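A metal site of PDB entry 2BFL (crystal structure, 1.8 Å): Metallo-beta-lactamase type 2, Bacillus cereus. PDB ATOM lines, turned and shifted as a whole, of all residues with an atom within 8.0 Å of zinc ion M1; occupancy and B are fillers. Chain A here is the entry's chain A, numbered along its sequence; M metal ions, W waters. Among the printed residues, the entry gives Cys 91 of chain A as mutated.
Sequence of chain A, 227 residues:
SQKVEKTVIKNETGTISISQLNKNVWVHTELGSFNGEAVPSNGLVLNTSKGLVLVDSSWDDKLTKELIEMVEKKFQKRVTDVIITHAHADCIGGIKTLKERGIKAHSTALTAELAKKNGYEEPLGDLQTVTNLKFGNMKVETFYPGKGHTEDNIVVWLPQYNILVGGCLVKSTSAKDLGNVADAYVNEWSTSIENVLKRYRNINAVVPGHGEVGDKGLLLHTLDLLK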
ATOM      1  N   TRP A  59      24.201  -8.723 -16.325  1.00  0.00           N
ATOM      2  CA  TRP A  59      23.679  -7.617 -17.135  1.00  0.00           C
ATOM      3  C   TRP A  59      24.660  -6.504 -17.478  1.00  0.00           C
ATOM      4  O   TRP A  59      24.680  -6.028 -18.599  1.00  0.00           O
ATOM      5  CB  TRP A  59      22.455  -7.002 -16.459  1.00  0.00           C
ATOM      6  CG  TRP A  59      21.311  -7.955 -16.319  1.00  0.00           C
ATOM      7  CD1 TRP A  59      21.009  -8.738 -15.240  1.00  0.00           C
ATOM      8  CD2 TRP A  59      20.289  -8.209 -17.303  1.00  0.00           C
ATOM      9  NE1 TRP A  59      19.864  -9.454 -15.488  1.00  0.00           N
ATOM     10  CE2 TRP A  59      19.402  -9.148 -16.741  1.00  0.00           C
ATOM     11  CE3 TRP A  59      20.041  -7.732 -18.599  1.00  0.00           C
ATOM     12  CZ2 TRP A  59      18.277  -9.634 -17.427  1.00  0.00           C
ATOM     13  CZ3 TRP A  59      18.924  -8.203 -19.282  1.00  0.00           C
ATOM     14  CH2 TRP A  59      18.058  -9.145 -18.696  1.00  0.00           C
ATOM     15  N   THR A  85      27.512 -17.705 -23.284  1.00  0.00           N
ATOM     16  CA  THR A  85      26.611 -18.481 -24.148  1.00  0.00           C
ATOM     17  C   THR A  85      26.098 -17.739 -25.391  1.00  0.00           C
ATOM     18  O   THR A  85      25.765 -18.375 -26.397  1.00  0.00           O
ATOM     19  CB  THR A  85      25.451 -19.074 -23.336  1.00  0.00           C
ATOM     20  OG1 THR A  85      24.675 -18.027 -22.742  1.00  0.00           O
ATOM     21  CG2 THR A  85      25.997 -19.970 -22.243  1.00  0.00           C
ATOM     22  N   HIS A  86      26.013 -16.412 -25.317  1.00  0.00           N
ATOM     23  CA  HIS A  86      25.630 -15.593 -26.480  1.00  0.00           C
ATOM     24  C   HIS A  86      25.896 -14.114 -26.221  1.00  0.00           C
ATOM     25  O   HIS A  86      26.146 -13.708 -25.090  1.00  0.00           O
ATOM     26  CB  HIS A  86      24.185 -15.844 -26.938  1.00  0.00           C
ATOM     27  CG  HIS A  86      23.128 -15.312 -26.028  1.00  0.00           C
ATOM     28  ND1 HIS A  86      22.838 -15.884 -24.804  1.00  0.00           N
ATOM     29  CD2 HIS A  86      22.234 -14.308 -26.188  1.00  0.00           C
ATOM     30  CE1 HIS A  86      21.814 -15.261 -24.264  1.00  0.00           C
ATOM     31  NE2 HIS A  86      21.423 -14.290 -25.085  1.00  0.00           N
ATOM     32  N   ALA A  87      25.865 -13.322 -27.285  1.00  0.00           N
ATOM     33  CA  ALA A  87      26.164 -11.888 -27.234  1.00  0.00           C
ATOM     34  C   ALA A  87      25.077 -10.884 -26.813  1.00  0.00           C
ATOM     35  O   ALA A  87      24.943  -9.824 -27.422  1.00  0.00           O
ATOM     36  CB  ALA A  87      26.758 -11.451 -28.575  1.00  0.00           C
ATOM     37  N   HIS A  88      24.313 -11.216 -25.782  1.00  0.00           N
ATOM     38  CA  HIS A  88      23.291 -10.306 -25.265  1.00  0.00           C
ATOM     39  C   HIS A  88      23.760  -9.835 -23.878  1.00  0.00           C
ATOM     40  O   HIS A  88      24.552 -10.522 -23.224  1.00  0.00           O
ATOM     41  CB  HIS A  88      21.917 -10.997 -25.157  1.00  0.00           C
ATOM     42  CG  HIS A  88      21.114 -10.944 -26.410  1.00  0.00           C
ATOM     43  ND1 HIS A  88      19.970 -11.702 -26.602  1.00  0.00           N
ATOM     44  CD2 HIS A  88      21.285 -10.241 -27.557  1.00  0.00           C
ATOM     45  CE1 HIS A  88      19.476 -11.455 -27.797  1.00  0.00           C
ATOM     46  NE2 HIS A  88      20.252 -10.567 -28.397  1.00  0.00           N
ATOM     47  N   ALA A  89      23.268  -8.677 -23.448  1.00  0.00           N
ATOM     48  CA  ALA A  89      23.643  -8.106 -22.154  1.00  0.00           C
ATOM     49  C   ALA A  89      23.605  -9.043 -20.952  1.00  0.00           C
ATOM     50  O   ALA A  89      24.556  -9.100 -20.176  1.00  0.00           O
ATOM     51  CB  ALA A  89      22.793  -6.872 -21.864  1.00  0.00           C
ATOM     52  N   ASP A  90      22.511  -9.793 -20.789  1.00  0.00           N
ATOM     53  CA  ASP A  90      22.396 -10.693 -19.653  1.00  0.00           C
ATOM     54  C   ASP A  90      23.466 -11.793 -19.616  1.00  0.00           C
ATOM     55  O   ASP A  90      23.605 -12.499 -18.617  1.00  0.00           O
ATOM     56  CB  ASP A  90      20.985 -11.307 -19.585  1.00  0.00           C
ATOM     57  CG  ASP A  90      20.678 -12.223 -20.759  1.00  0.00           C
ATOM     58  OD1 ASP A  90      21.056 -11.900 -21.908  1.00  0.00           O
ATOM     59  OD2 ASP A  90      20.018 -13.267 -20.548  1.00  0.00           O
ATOM     60  N   CYS A  91      24.223 -11.919 -20.710  1.00  0.00           N
ATOM     61  CA  CYS A  91      25.283 -12.937 -20.817  1.00  0.00           C
ATOM     62  C   CYS A  91      26.692 -12.368 -20.888  1.00  0.00           C
ATOM     63  O   CYS A  91      27.609 -12.858 -20.210  1.00  0.00           O
ATOM     64  CB  CYS A  91      25.044 -13.822 -22.043  1.00  0.00           C
ATOM     65  SG  CYS A  91      23.685 -14.981 -21.853  1.00  0.00           S
ATOM     66  N   HIS A 149      17.364 -18.662 -30.232  1.00  0.00           N
ATOM     67  CA  HIS A 149      17.110 -17.397 -29.543  1.00  0.00           C
ATOM     68  C   HIS A 149      17.953 -16.316 -30.227  1.00  0.00           C
ATOM     69  O   HIS A 149      17.527 -15.175 -30.388  1.00  0.00           O
ATOM     70  CB  HIS A 149      17.500 -17.534 -28.069  1.00  0.00           C
ATOM     71  CG  HIS A 149      17.549 -16.232 -27.347  1.00  0.00           C
ATOM     72  ND1 HIS A 149      16.431 -15.423 -27.172  1.00  0.00           N
ATOM     73  CD2 HIS A 149      18.580 -15.560 -26.794  1.00  0.00           C
ATOM     74  CE1 HIS A 149      16.782 -14.327 -26.552  1.00  0.00           C
ATOM     75  NE2 HIS A 149      18.083 -14.367 -26.306  1.00  0.00           N
ATOM     76  N   THR A 150      19.170 -16.695 -30.603  1.00  0.00           N
ATOM     77  CA  THR A 150      20.082 -15.822 -31.328  1.00  0.00           C
ATOM     78  C   THR A 150      20.800 -16.704 -32.331  1.00  0.00           C
ATOM     79  O   THR A 150      20.693 -17.928 -32.297  1.00  0.00           O
ATOM     80  CB  THR A 150      21.151 -15.148 -30.422  1.00  0.00           C
ATOM     81  OG1 THR A 150      21.893 -16.138 -29.710  1.00  0.00           O
ATOM     82  CG2 THR A 150      20.509 -14.202 -29.434  1.00  0.00           C
ATOM     83  N   ASP A 152      23.962 -17.151 -32.511  1.00  0.00           N
ATOM     84  CA  ASP A 152      25.127 -17.757 -31.879  1.00  0.00           C
ATOM     85  C   ASP A 152      24.956 -18.580 -30.611  1.00  0.00           C
ATOM     86  O   ASP A 152      25.932 -19.149 -30.116  1.00  0.00           O
ATOM     87  CB  ASP A 152      26.164 -16.658 -31.609  1.00  0.00           C
ATOM     88  CG  ASP A 152      25.670 -15.617 -30.593  1.00  0.00           C
ATOM     89  OD1 ASP A 152      24.513 -15.158 -30.725  1.00  0.00           O
ATOM     90  OD2 ASP A 152      26.429 -15.250 -29.674  1.00  0.00           O
ATOM     91  N   ASN A 153      23.745 -18.652 -30.064  1.00  0.00           N
ATOM     92  CA  ASN A 153      23.550 -19.381 -28.824  1.00  0.00           C
ATOM     93  C   ASN A 153      24.116 -20.803 -28.726  1.00  0.00           C
ATOM     94  O   ASN A 153      23.977 -21.614 -29.643  1.00  0.00           O
ATOM     95  CB  ASN A 153      22.049 -19.364 -28.429  1.00  0.00           C
ATOM     96  CG  ASN A 153      21.127 -19.880 -29.527  1.00  0.00           C
ATOM     97  OD1 ASN A 153      19.944 -19.527 -29.559  1.00  0.00           O
ATOM     98  ND2 ASN A 153      21.631 -20.729 -30.416  1.00  0.00           N
ATOM     99  N   GLY A 167      20.281 -21.858 -21.312  1.00  0.00           N
ATOM    100  CA  GLY A 167      20.375 -20.453 -21.630  1.00  0.00           C
ATOM    101  C   GLY A 167      19.047 -19.976 -22.176  1.00  0.00           C
ATOM    102  O   GLY A 167      18.010 -20.585 -21.919  1.00  0.00           O
ATOM    103  N   CYS A 168      19.056 -18.909 -22.956  1.00  0.00           N
ATOM    104  CA  CYS A 168      17.823 -18.386 -23.489  1.00  0.00           C
ATOM    105  C   CYS A 168      17.196 -19.223 -24.611  1.00  0.00           C
ATOM    106  O   CYS A 168      16.145 -18.869 -25.135  1.00  0.00           O
ATOM    107  CB  CYS A 168      18.044 -16.945 -23.924  1.00  0.00           C
ATOM    108  SG  CYS A 168      18.531 -15.953 -22.482  1.00  0.00           S
ATOM    109  N   LEU A 169      17.837 -20.329 -24.956  1.00  0.00           N
ATOM    110  CA  LEU A 169      17.315 -21.230 -25.977  1.00  0.00           C
ATOM    111  C   LEU A 169      16.166 -22.018 -25.341  1.00  0.00           C
ATOM    112  O   LEU A 169      15.325 -22.597 -26.028  1.00  0.00           O
ATOM    113  CB  LEU A 169      18.397 -22.208 -26.436  1.00  0.00           C
ATOM    114  CG  LEU A 169      18.067 -23.098 -27.637  1.00  0.00           C
ATOM    115  CD1 LEU A 169      18.143 -22.297 -28.934  1.00  0.00           C
ATOM    116  CD2 LEU A 169      19.034 -24.261 -27.689  1.00  0.00           C
ATOM    117  N   LYS A 171      13.033 -21.904 -22.417  1.00  0.00           N
ATOM    118  CA  LYS A 171      12.176 -21.082 -21.565  1.00  0.00           C
ATOM    119  C   LYS A 171      11.744 -21.863 -20.325  1.00  0.00           C
ATOM    120  O   LYS A 171      11.653 -23.094 -20.349  1.00  0.00           O
ATOM    121  CB  LYS A 171      10.934 -20.620 -22.336  1.00  0.00           C
ATOM    122  CG  LYS A 171      11.218 -20.059 -23.738  1.00  0.00           C
ATOM    123  CD  LYS A 171      12.265 -18.950 -23.733  1.00  0.00           C
ATOM    124  CE  LYS A 171      11.784 -17.702 -23.023  1.00  0.00           C
ATOM    125  NZ  LYS A 171      12.787 -16.615 -23.181  1.00  0.00           N
ATOM    126  N   LEU A 178       8.393 -15.980 -25.776  1.00  0.00           N
ATOM    127  CA  LEU A 178       9.728 -16.355 -26.232  1.00  0.00           C
ATOM    128  C   LEU A 178      10.776 -15.277 -25.930  1.00  0.00           C
ATOM    129  O   LEU A 178      11.980 -15.557 -25.938  1.00  0.00           O
ATOM    130  CB  LEU A 178       9.726 -16.651 -27.735  1.00  0.00           C
ATOM    131  CG  LEU A 178       8.954 -17.896 -28.178  1.00  0.00           C
ATOM    132  CD1 LEU A 178       8.814 -17.897 -29.695  1.00  0.00           C
ATOM    133  CD2 LEU A 178       9.685 -19.132 -27.691  1.00  0.00           C
ATOM    134  N   ASN A 180      12.723 -11.545 -26.673  1.00  0.00           N
ATOM    135  CA  ASN A 180      13.144 -10.758 -27.833  1.00  0.00           C
ATOM    136  C   ASN A 180      13.390 -11.697 -29.008  1.00  0.00           C
ATOM    137  O   ASN A 180      14.278 -12.544 -28.948  1.00  0.00           O
ATOM    138  CB  ASN A 180      14.439 -10.011 -27.496  1.00  0.00           C
ATOM    139  CG  ASN A 180      14.947  -9.157 -28.654  1.00  0.00           C
ATOM    140  OD1 ASN A 180      14.848  -9.528 -29.820  1.00  0.00           O
ATOM    141  ND2 ASN A 180      15.523  -8.008 -28.318  1.00  0.00           N
ATOM    142  N   ASP A 183      16.296 -10.660 -32.888  1.00  0.00           N
ATOM    143  CA  ASP A 183      17.582 -11.254 -33.255  1.00  0.00           C
ATOM    144  C   ASP A 183      17.473 -12.782 -33.318  1.00  0.00           C
ATOM    145  O   ASP A 183      18.479 -13.480 -33.476  1.00  0.00           O
ATOM    146  CB  ASP A 183      18.661 -10.909 -32.218  1.00  0.00           C
ATOM    147  CG  ASP A 183      18.823  -9.420 -32.011  1.00  0.00           C
ATOM    148  OD1 ASP A 183      18.603  -8.648 -32.970  1.00  0.00           O
ATOM    149  OD2 ASP A 183      19.176  -9.028 -30.886  1.00  0.00           O
ATOM    150  N   HIS A 210      16.174 -17.834 -17.875  1.00  0.00           N
ATOM    151  CA  HIS A 210      15.484 -17.078 -16.830  1.00  0.00           C
ATOM    152  C   HIS A 210      14.459 -18.057 -16.239  1.00  0.00           C
ATOM    153  O   HIS A 210      13.816 -18.811 -16.976  1.00  0.00           O
ATOM    154  CB  HIS A 210      14.732 -15.883 -17.429  1.00  0.00           C
ATOM    155  CG  HIS A 210      15.574 -15.011 -18.314  1.00  0.00           C
ATOM    156  ND1 HIS A 210      16.480 -14.090 -17.812  1.00  0.00           N
ATOM    157  CD2 HIS A 210      15.628 -14.893 -19.656  1.00  0.00           C
ATOM    158  CE1 HIS A 210      17.042 -13.445 -18.818  1.00  0.00           C
ATOM    159  NE2 HIS A 210      16.548 -13.909 -19.945  1.00  0.00           N
HETATM  160 ZN    ZN M   1      19.517 -13.207 -25.364  1.00  0.00          ZN
HETATM  161 ZN    ZN M   2      16.804 -14.528 -22.375  1.00  0.00          ZN
HETATM  162  O   HOH W   1      17.599 -11.244 -24.954  1.00  0.00           O
HETATM  163  O   HOH W   2      19.351 -13.305 -23.291  1.00  0.00           O
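Zinc ion M1 is bound by a ring nitrogen (ND1) of His 88, a ring nitrogen (NE2) of His 149, water W2 and a ring nitrogen (NE2) of His 86. Slightly farther from zinc ion M1 lies water W1 (2.8 Å).
A ring nitrogen (NE2) of His 88 sits at hydrogen-bond distance from the side-chain carboxylate (OD2) of Asp 183 (3.1 Å). The side-chain amide oxygen (OD1) of Asn 153 lies within hydrogen-bond range of the backbone NH (N) of His 149 (2.8 Å). A ring nitrogen (ND1) of His 86 lies close to the side-chain sulfur (SG) of Cys 91, at 3.2 Å. A ring nitrogen (ND1) of His 86 lies within hydrogen-bond range of the side-chain hydroxyl (OG1) of Thr 85, at 3.5 Å.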
